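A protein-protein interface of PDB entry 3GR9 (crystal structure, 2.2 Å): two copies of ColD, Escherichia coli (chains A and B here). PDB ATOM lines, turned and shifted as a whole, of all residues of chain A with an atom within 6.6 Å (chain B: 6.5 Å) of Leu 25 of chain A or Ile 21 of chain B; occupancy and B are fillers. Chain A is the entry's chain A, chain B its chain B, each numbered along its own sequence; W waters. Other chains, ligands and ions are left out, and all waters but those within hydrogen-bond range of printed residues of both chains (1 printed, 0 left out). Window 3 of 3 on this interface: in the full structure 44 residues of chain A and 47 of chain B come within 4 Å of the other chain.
Tyr 18 of chain A touches Leu 25 of chain B, but with the chains exchanged Leu 25 of chain A does not touch Tyr 18 of chain B (4.1 Å).
Leu 25 of chain A touches Ile 21 of chain B, but with the chains exchanged Ile 21 of chain A does not touch Leu 25 of chain B (4.5 Å).
Met 256 of chain B touches its own counterpart, Met 256 of chain A.
Leu 25 of chain A touches just one residue of chain B: Ile 21.
Ile 21 of chain B touches just one residue of chain A: Leu 25 (3.96 Å).
Of the printed residues of chain B, Lys 28 of chain A touches Tyr 18.
Of the printed residues of chain B, Phe 30 of chain A touches Trp 13, Tyr 18 and Met 195.
Of the printed residues of chain A, Met 195 of chain B touches Phe 30.
Of the printed residues of chain B, Tyr 18 of chain A touches Leu 25 (3.2 Å).
Of the printed residues of chain A, Trp 13 of chain B touches Phe 30 (3.7 Å).
Ala 20 of chain B touches none of the printed residues of chain A.
Leu 25 of chain B touches Tyr 18 of chain A (CD2 to CE1, 3.2 Å).
Leu 25 of chain A touches Ile 21 of chain B (CD2 to CD1, 3.96 Å).
Lys 28 of chain A touches Tyr 18 of chain B (CD to OH, 3.2 Å).
Trp 13 of chain B touches Phe 30 of chain A.
OH of Tyr 18 of chain B touches CZ of Phe 30 of chain A, at 3.5 Å.
Phe 30 of chain A touches Met 195 of chain B (CB to SD, 3.4 Å).
Water W1 lies within hydrogen-bond range of O of Phe 30 of chain A, N of Met 256 of chain A and SD of Met 195 of chain B.
Of the 16 printed residues of chain B, 6 touch a printed residue of chain A.
Of the 13 printed residues of chain A, 5 touch a printed residue of chain B.
Printed residues of chain A that touch a printed residue of chain B: Tyr 18, Leu 25, Lys 28, Phe 30 and Met 256.
Hydrophobic or aromatic side chains of chain A that line the printed part of chain B: Tyr 18, Leu 25, Phe 30 and Met 256.
Among the printed residues, 7 pairs touch across the chains.
Among the printed residues, no Asp or Glu carboxylate lies within 4 Å of a Lys or Arg side-chain nitrogen of the other chain.
The side-chain sulfur (SD) of Met 256 of chain A lies close to the side-chain sulfur (SD) of Met 256 of chain B.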
ATOM      1  N   TYR A  18     -10.327  21.284  23.976  1.00  0.00           N
ATOM      2  CA  TYR A  18     -11.761  21.466  24.174  1.00  0.00           C
ATOM      3  C   TYR A  18     -12.447  21.537  22.789  1.00  0.00           C
ATOM      4  O   TYR A  18     -13.481  20.879  22.566  1.00  0.00           O
ATOM      5  CB  TYR A  18     -12.034  22.693  25.046  1.00  0.00           C
ATOM      6  CG  TYR A  18     -12.003  22.348  26.522  1.00  0.00           C
ATOM      7  CD1 TYR A  18     -13.105  21.739  27.134  1.00  0.00           C
ATOM      8  CD2 TYR A  18     -10.888  22.659  27.304  1.00  0.00           C
ATOM      9  CE1 TYR A  18     -13.086  21.430  28.475  1.00  0.00           C
ATOM     10  CE2 TYR A  18     -10.854  22.350  28.652  1.00  0.00           C
ATOM     11  CZ  TYR A  18     -11.960  21.740  29.233  1.00  0.00           C
ATOM     12  OH  TYR A  18     -11.920  21.418  30.570  1.00  0.00           O
ATOM     13  N   ALA A  20     -11.341  20.329  19.932  1.00  0.00           N
ATOM     14  CA  ALA A  20     -11.316  19.001  19.295  1.00  0.00           C
ATOM     15  C   ALA A  20     -12.533  18.234  19.726  1.00  0.00           C
ATOM     16  O   ALA A  20     -13.211  17.606  18.903  1.00  0.00           O
ATOM     17  CB  ALA A  20     -10.116  18.262  19.712  1.00  0.00           C
ATOM     18  N   ILE A  21     -12.831  18.340  21.013  1.00  0.00           N
ATOM     19  CA  ILE A  21     -13.993  17.614  21.500  1.00  0.00           C
ATOM     20  C   ILE A  21     -15.280  18.008  20.812  1.00  0.00           C
ATOM     21  O   ILE A  21     -16.090  17.146  20.422  1.00  0.00           O
ATOM     22  CB  ILE A  21     -14.113  17.714  23.028  1.00  0.00           C
ATOM     23  CG1 ILE A  21     -12.872  17.069  23.696  1.00  0.00           C
ATOM     24  CG2 ILE A  21     -15.355  16.980  23.570  1.00  0.00           C
ATOM     25  CD1 ILE A  21     -12.819  17.308  25.194  1.00  0.00           C
ATOM     26  N   GLN A  22     -15.478  19.304  20.609  1.00  0.00           N
ATOM     27  CA  GLN A  22     -16.706  19.731  19.945  1.00  0.00           C
ATOM     28  C   GLN A  22     -16.783  19.047  18.620  1.00  0.00           C
ATOM     29  O   GLN A  22     -17.821  18.510  18.224  1.00  0.00           O
ATOM     30  CB  GLN A  22     -16.668  21.208  19.627  1.00  0.00           C
ATOM     31  CG  GLN A  22     -18.025  21.663  19.218  1.00  0.00           C
ATOM     32  CD  GLN A  22     -19.046  21.382  20.309  1.00  0.00           C
ATOM     33  OE1 GLN A  22     -18.893  21.851  21.444  1.00  0.00           O
ATOM     34  NE2 GLN A  22     -20.085  20.606  19.980  1.00  0.00           N
ATOM     35  N   SER A  23     -15.668  19.156  17.911  1.00  0.00           N
ATOM     36  CA  SER A  23     -15.575  18.604  16.576  1.00  0.00           C
ATOM     37  C   SER A  23     -16.155  17.210  16.461  1.00  0.00           C
ATOM     38  O   SER A  23     -16.840  16.900  15.477  1.00  0.00           O
ATOM     39  CB  SER A  23     -14.141  18.662  16.089  1.00  0.00           C
ATOM     40  OG  SER A  23     -14.006  19.705  15.143  1.00  0.00           O
ATOM     41  N   VAL A  24     -15.888  16.394  17.482  1.00  0.00           N
ATOM     42  CA  VAL A  24     -16.352  15.018  17.550  1.00  0.00           C
ATOM     43  C   VAL A  24     -17.844  15.043  17.860  1.00  0.00           C
ATOM     44  O   VAL A  24     -18.658  14.247  17.373  1.00  0.00           O
ATOM     45  CB  VAL A  24     -15.641  14.291  18.708  1.00  0.00           C
ATOM     46  CG1 VAL A  24     -16.116  12.844  18.800  1.00  0.00           C
ATOM     47  CG2 VAL A  24     -14.121  14.370  18.565  1.00  0.00           C
ATOM     48  N   LEU A  25     -18.222  15.981  18.692  1.00  0.00           N
ATOM     49  CA  LEU A  25     -19.624  16.022  19.008  1.00  0.00           C
ATOM     50  C   LEU A  25     -20.312  16.308  17.703  1.00  0.00           C
ATOM     51  O   LEU A  25     -21.254  15.604  17.321  1.00  0.00           O
ATOM     52  CB  LEU A  25     -19.927  17.087  20.050  1.00  0.00           C
ATOM     53  CG  LEU A  25     -19.298  16.733  21.399  1.00  0.00           C
ATOM     54  CD1 LEU A  25     -19.246  17.968  22.277  1.00  0.00           C
ATOM     55  CD2 LEU A  25     -20.120  15.625  22.070  1.00  0.00           C
ATOM     56  N   ASP A  26     -19.828  17.352  17.029  1.00  0.00           N
ATOM     57  CA  ASP A  26     -20.372  17.821  15.754  1.00  0.00           C
ATOM     58  C   ASP A  26     -20.475  16.765  14.685  1.00  0.00           C
ATOM     59  O   ASP A  26     -21.491  16.687  13.980  1.00  0.00           O
ATOM     60  CB  ASP A  26     -19.486  18.912  15.187  1.00  0.00           C
ATOM     61  CG  ASP A  26     -19.644  20.225  15.909  1.00  0.00           C
ATOM     62  OD1 ASP A  26     -20.554  20.320  16.799  1.00  0.00           O
ATOM     63  OD2 ASP A  26     -18.824  21.127  15.591  1.00  0.00           O
ATOM     64  N   SER A  27     -19.394  16.022  14.483  1.00  0.00           N
ATOM     65  CA  SER A  27     -19.446  14.978  13.476  1.00  0.00           C
ATOM     66  C   SER A  27     -20.467  13.930  13.985  1.00  0.00           C
ATOM     67  O   SER A  27     -20.944  13.067  13.242  1.00  0.00           O
ATOM     68  CB  SER A  27     -18.080  14.296  13.375  1.00  0.00           C
ATOM     69  OG  SER A  27     -17.875  13.370  14.444  1.00  0.00           O
ATOM     70  N   LYS A  28     -20.758  13.949  15.279  1.00  0.00           N
ATOM     71  CA  LYS A  28     -21.711  12.984  15.854  1.00  0.00           C
ATOM     72  C   LYS A  28     -21.249  11.545  15.648  1.00  0.00           C
ATOM     73  O   LYS A  28     -22.049  10.651  15.336  1.00  0.00           O
ATOM     74  CB  LYS A  28     -23.074  13.134  15.172  1.00  0.00           C
ATOM     75  CG  LYS A  28     -23.497  14.562  14.926  1.00  0.00           C
ATOM     76  CD  LYS A  28     -24.563  14.957  15.926  1.00  0.00           C
ATOM     77  CE  LYS A  28     -24.787  16.444  15.983  1.00  0.00           C
ATOM     78  NZ  LYS A  28     -26.183  16.666  15.468  1.00  0.00           N
ATOM     79  N   MET A  29     -19.955  11.309  15.787  1.00  0.00           N
ATOM     80  CA  MET A  29     -19.422   9.965  15.572  1.00  0.00           C
ATOM     81  C   MET A  29     -18.448   9.662  16.704  1.00  0.00           C
ATOM     82  O   MET A  29     -17.267  10.008  16.656  1.00  0.00           O
ATOM     83  CB  MET A  29     -18.694   9.975  14.230  1.00  0.00           C
ATOM     84  CG  MET A  29     -19.352   9.118  13.171  1.00  0.00           C
ATOM     85  SD  MET A  29     -20.736   9.940  12.308  1.00  0.00           S
ATOM     86  CE  MET A  29     -20.825   8.919  10.698  1.00  0.00           C
ATOM     87  N   PHE A  30     -18.957   9.000  17.730  1.00  0.00           N
ATOM     88  CA  PHE A  30     -18.181   8.766  18.929  1.00  0.00           C
ATOM     89  C   PHE A  30     -17.433   7.441  19.104  1.00  0.00           C
ATOM     90  O   PHE A  30     -16.583   7.305  20.010  1.00  0.00           O
ATOM     91  CB  PHE A  30     -19.000   9.221  20.134  1.00  0.00           C
ATOM     92  CG  PHE A  30     -20.062  10.207  19.764  1.00  0.00           C
ATOM     93  CD1 PHE A  30     -19.740  11.540  19.589  1.00  0.00           C
ATOM     94  CD2 PHE A  30     -21.360   9.781  19.500  1.00  0.00           C
ATOM     95  CE1 PHE A  30     -20.706  12.445  19.190  1.00  0.00           C
ATOM     96  CE2 PHE A  30     -22.333  10.681  19.116  1.00  0.00           C
ATOM     97  CZ  PHE A  30     -22.008  12.011  18.947  1.00  0.00           C
ATOM     98  N   MET A 256     -13.311  10.508  20.683  1.00  0.00           N
ATOM     99  CA  MET A 256     -13.000  11.707  21.483  1.00  0.00           C
ATOM    100  C   MET A 256     -11.602  11.605  22.071  1.00  0.00           C
ATOM    101  O   MET A 256     -10.871  12.611  22.177  1.00  0.00           O
ATOM    102  CB  MET A 256     -13.999  11.808  22.622  1.00  0.00           C
ATOM    103  CG  MET A 256     -14.521  13.201  22.888  1.00  0.00           C
ATOM    104  SD  MET A 256     -15.716  13.108  24.230  1.00  0.00           S
ATOM    105  CE  MET A 256     -17.227  13.685  23.238  1.00  0.00           C
ATOM    106  N   TRP B  13     -29.972   9.857  21.376  1.00  0.00           N
ATOM    107  CA  TRP B  13     -29.628  11.074  22.115  1.00  0.00           C
ATOM    108  C   TRP B  13     -30.483  12.299  21.807  1.00  0.00           C
ATOM    109  O   TRP B  13     -31.140  12.377  20.758  1.00  0.00           O
ATOM    110  CB  TRP B  13     -28.196  11.483  21.730  1.00  0.00           C
ATOM    111  CG  TRP B  13     -27.132  10.652  22.343  1.00  0.00           C
ATOM    112  CD1 TRP B  13     -27.309   9.447  22.949  1.00  0.00           C
ATOM    113  CD2 TRP B  13     -25.742  10.972  22.463  1.00  0.00           C
ATOM    114  NE1 TRP B  13     -26.107   8.960  23.391  1.00  0.00           N
ATOM    115  CE2 TRP B  13     -25.135   9.885  23.128  1.00  0.00           C
ATOM    116  CE3 TRP B  13     -24.947  12.064  22.076  1.00  0.00           C
ATOM    117  CZ2 TRP B  13     -23.758   9.851  23.411  1.00  0.00           C
ATOM    118  CZ3 TRP B  13     -23.606  12.026  22.355  1.00  0.00           C
ATOM    119  CH2 TRP B  13     -23.025  10.928  23.025  1.00  0.00           C
ATOM    120  N   LEU B  16     -30.250  16.764  25.928  1.00  0.00           N
ATOM    121  CA  LEU B  16     -29.975  16.369  27.294  1.00  0.00           C
ATOM    122  C   LEU B  16     -28.650  15.665  27.424  1.00  0.00           C
ATOM    123  O   LEU B  16     -27.846  15.956  28.337  1.00  0.00           O
ATOM    124  CB  LEU B  16     -31.117  15.515  27.815  1.00  0.00           C
ATOM    125  CG  LEU B  16     -32.392  16.407  27.943  1.00  0.00           C
ATOM    126  CD1 LEU B  16     -33.679  15.573  27.813  1.00  0.00           C
ATOM    127  CD2 LEU B  16     -32.327  17.157  29.319  1.00  0.00           C
ATOM    128  N   GLU B  17     -28.379  14.761  26.498  1.00  0.00           N
ATOM    129  CA  GLU B  17     -27.096  14.092  26.559  1.00  0.00           C
ATOM    130  C   GLU B  17     -26.010  15.134  26.291  1.00  0.00           C
ATOM    131  O   GLU B  17     -25.052  15.311  27.047  1.00  0.00           O
ATOM    132  CB  GLU B  17     -27.092  12.990  25.517  1.00  0.00           C
ATOM    133  CG  GLU B  17     -27.883  11.791  26.019  1.00  0.00           C
ATOM    134  CD  GLU B  17     -29.368  11.949  25.786  1.00  0.00           C
ATOM    135  OE1 GLU B  17     -29.723  12.751  24.901  1.00  0.00           O
ATOM    136  OE2 GLU B  17     -30.173  11.261  26.466  1.00  0.00           O
ATOM    137  N   TYR B  18     -26.190  15.895  25.230  1.00  0.00           N
ATOM    138  CA  TYR B  18     -25.188  16.899  24.924  1.00  0.00           C
ATOM    139  C   TYR B  18     -24.798  17.854  26.085  1.00  0.00           C
ATOM    140  O   TYR B  18     -23.616  18.149  26.338  1.00  0.00           O
ATOM    141  CB  TYR B  18     -25.453  17.552  23.546  1.00  0.00           C
ATOM    142  CG  TYR B  18     -25.289  16.617  22.338  1.00  0.00           C
ATOM    143  CD1 TYR B  18     -26.250  15.649  22.062  1.00  0.00           C
ATOM    144  CD2 TYR B  18     -24.207  16.770  21.446  1.00  0.00           C
ATOM    145  CE1 TYR B  18     -26.107  14.801  20.974  1.00  0.00           C
ATOM    146  CE2 TYR B  18     -24.037  15.922  20.356  1.00  0.00           C
ATOM    147  CZ  TYR B  18     -24.995  14.937  20.131  1.00  0.00           C
ATOM    148  OH  TYR B  18     -24.877  14.095  19.038  1.00  0.00           O
ATOM    149  N   LYS B  19     -25.765  18.313  26.867  1.00  0.00           N
ATOM    150  CA  LYS B  19     -25.372  19.224  27.958  1.00  0.00           C
ATOM    151  C   LYS B  19     -24.842  18.383  29.100  1.00  0.00           C
ATOM    152  O   LYS B  19     -24.114  18.891  29.948  1.00  0.00           O
ATOM    153  CB  LYS B  19     -26.506  20.104  28.453  1.00  0.00           C
ATOM    154  CG  LYS B  19     -27.821  19.781  27.790  1.00  0.00           C
ATOM    155  CD  LYS B  19     -28.895  20.754  28.237  1.00  0.00           C
ATOM    156  CE  LYS B  19     -29.743  20.202  29.420  1.00  0.00           C
ATOM    157  NZ  LYS B  19     -31.214  20.224  29.137  1.00  0.00           N
ATOM    158  N   ALA B  20     -25.153  17.089  29.080  1.00  0.00           N
ATOM    159  CA  ALA B  20     -24.628  16.204  30.107  1.00  0.00           C
ATOM    160  C   ALA B  20     -23.125  16.177  29.893  1.00  0.00           C
ATOM    161  O   ALA B  20     -22.323  16.233  30.840  1.00  0.00           O
ATOM    162  CB  ALA B  20     -25.216  14.831  29.935  1.00  0.00           C
ATOM    163  N   ILE B  21     -22.728  16.193  28.624  1.00  0.00           N
ATOM    164  CA  ILE B  21     -21.314  16.177  28.337  1.00  0.00           C
ATOM    165  C   ILE B  21     -20.777  17.528  28.736  1.00  0.00           C
ATOM    166  O   ILE B  21     -19.817  17.648  29.511  1.00  0.00           O
ATOM    167  CB  ILE B  21     -21.059  15.866  26.870  1.00  0.00           C
ATOM    168  CG1 ILE B  21     -21.461  14.425  26.603  1.00  0.00           C
ATOM    169  CG2 ILE B  21     -19.581  16.003  26.537  1.00  0.00           C
ATOM    170  CD1 ILE B  21     -22.015  14.182  25.228  1.00  0.00           C
ATOM    171  N   GLN B  22     -21.459  18.558  28.264  1.00  0.00           N
ATOM    172  CA  GLN B  22     -21.039  19.901  28.598  1.00  0.00           C
ATOM    173  C   GLN B  22     -20.680  20.001  30.074  1.00  0.00           C
ATOM    174  O   GLN B  22     -19.662  20.579  30.448  1.00  0.00           O
ATOM    175  CB  GLN B  22     -22.134  20.904  28.266  1.00  0.00           C
ATOM    176  CG  GLN B  22     -21.522  22.216  27.893  1.00  0.00           C
ATOM    177  CD  GLN B  22     -20.127  21.992  27.455  1.00  0.00           C
ATOM    178  OE1 GLN B  22     -19.890  21.273  26.476  1.00  0.00           O
ATOM    179  NE2 GLN B  22     -19.177  22.494  28.240  1.00  0.00           N
ATOM    180  N   SER B  23     -21.559  19.438  30.897  1.00  0.00           N
ATOM    181  CA  SER B  23     -21.430  19.438  32.348  1.00  0.00           C
ATOM    182  C   SER B  23     -20.193  18.741  32.885  1.00  0.00           C
ATOM    183  O   SER B  23     -19.560  19.220  33.835  1.00  0.00           O
ATOM    184  CB  SER B  23     -22.676  18.856  33.021  1.00  0.00           C
ATOM    185  OG  SER B  23     -23.796  18.874  32.157  1.00  0.00           O
ATOM    186  N   VAL B  24     -19.853  17.604  32.301  1.00  0.00           N
ATOM    187  CA  VAL B  24     -18.666  16.907  32.758  1.00  0.00           C
ATOM    188  C   VAL B  24     -17.441  17.721  32.395  1.00  0.00           C
ATOM    189  O   VAL B  24     -16.352  17.554  32.955  1.00  0.00           O
ATOM    190  CB  VAL B  24     -18.549  15.547  32.110  1.00  0.00           C
ATOM    191  CG1 VAL B  24     -17.123  15.038  32.237  1.00  0.00           C
ATOM    192  CG2 VAL B  24     -19.529  14.596  32.760  1.00  0.00           C
ATOM    193  N   LEU B  25     -17.602  18.587  31.409  1.00  0.00           N
ATOM    194  CA  LEU B  25     -16.487  19.420  30.978  1.00  0.00           C
ATOM    195  C   LEU B  25     -16.046  20.441  32.026  1.00  0.00           C
ATOM    196  O   LEU B  25     -14.901  20.453  32.501  1.00  0.00           O
ATOM    197  CB  LEU B  25     -16.900  20.119  29.703  1.00  0.00           C
ATOM    198  CG  LEU B  25     -16.471  19.243  28.541  1.00  0.00           C
ATOM    199  CD1 LEU B  25     -16.601  19.996  27.237  1.00  0.00           C
ATOM    200  CD2 LEU B  25     -15.027  18.843  28.760  1.00  0.00           C
ATOM    201  N   ASP B  26     -17.004  21.294  32.365  1.00  0.00           N
ATOM    202  CA  ASP B  26     -16.814  22.340  33.354  1.00  0.00           C
ATOM    203  C   ASP B  26     -16.364  21.786  34.681  1.00  0.00           C
ATOM    204  O   ASP B  26     -15.747  22.525  35.482  1.00  0.00           O
ATOM    205  CB  ASP B  26     -18.116  23.048  33.569  1.00  0.00           C
ATOM    206  CG  ASP B  26     -18.723  23.436  32.278  1.00  0.00           C
ATOM    207  OD1 ASP B  26     -18.377  22.756  31.285  1.00  0.00           O
ATOM    208  OD2 ASP B  26     -19.517  24.396  32.250  1.00  0.00           O
ATOM    209  N   MET B 195     -21.816   5.915  24.154  1.00  0.00           N
ATOM    210  CA  MET B 195     -20.618   5.865  23.302  1.00  0.00           C
ATOM    211  C   MET B 195     -20.120   4.432  23.577  1.00  0.00           C
ATOM    212  O   MET B 195     -20.536   3.491  22.904  1.00  0.00           O
ATOM    213  CB  MET B 195     -19.632   6.956  23.689  1.00  0.00           C
ATOM    214  CG  MET B 195     -20.189   8.366  23.508  1.00  0.00           C
ATOM    215  SD  MET B 195     -18.904   9.653  23.477  1.00  0.00           S
ATOM    216  CE  MET B 195     -18.227   9.681  25.253  1.00  0.00           C
ATOM    217  N   MET B 256     -17.843  10.887  31.467  1.00  0.00           N
ATOM    218  CA  MET B 256     -18.789  11.222  30.381  1.00  0.00           C
ATOM    219  C   MET B 256     -19.849  10.128  30.170  1.00  0.00           C
ATOM    220  O   MET B 256     -21.048  10.432  30.001  1.00  0.00           O
ATOM    221  CB  MET B 256     -18.093  11.558  29.040  1.00  0.00           C
ATOM    222  CG  MET B 256     -17.691  13.030  28.969  1.00  0.00           C
ATOM    223  SD  MET B 256     -16.579  13.468  27.635  1.00  0.00           S
ATOM    224  CE  MET B 256     -16.453  15.341  27.950  1.00  0.00           C
ATOM    225  N   ALA B 259     -22.261  10.188  33.045  1.00  0.00           N
ATOM    226  CA  ALA B 259     -23.233  11.247  32.871  1.00  0.00           C
ATOM    227  C   ALA B 259     -24.228  10.998  31.723  1.00  0.00           C
ATOM    228  O   ALA B 259     -25.395  11.353  31.829  1.00  0.00           O
ATOM    229  CB  ALA B 259     -22.545  12.586  32.726  1.00  0.00           C
ATOM    230  N   ILE B 260     -23.786  10.405  30.617  1.00  0.00           N
ATOM    231  CA  ILE B 260     -24.725  10.170  29.515  1.00  0.00           C
ATOM    232  C   ILE B 260     -25.726   9.100  29.862  1.00  0.00           C
ATOM    233  O   ILE B 260     -26.922   9.255  29.556  1.00  0.00           O
ATOM    234  CB  ILE B 260     -24.070   9.869  28.195  1.00  0.00           C
ATOM    235  CG1 ILE B 260     -22.937  10.865  27.955  1.00  0.00           C
ATOM    236  CG2 ILE B 260     -25.077  10.036  27.096  1.00  0.00           C
ATOM    237  CD1 ILE B 260     -21.780  10.263  27.086  1.00  0.00           C
HETATM  238  O   HOH W   1     -16.082   9.592  21.385  1.00  0.00           O
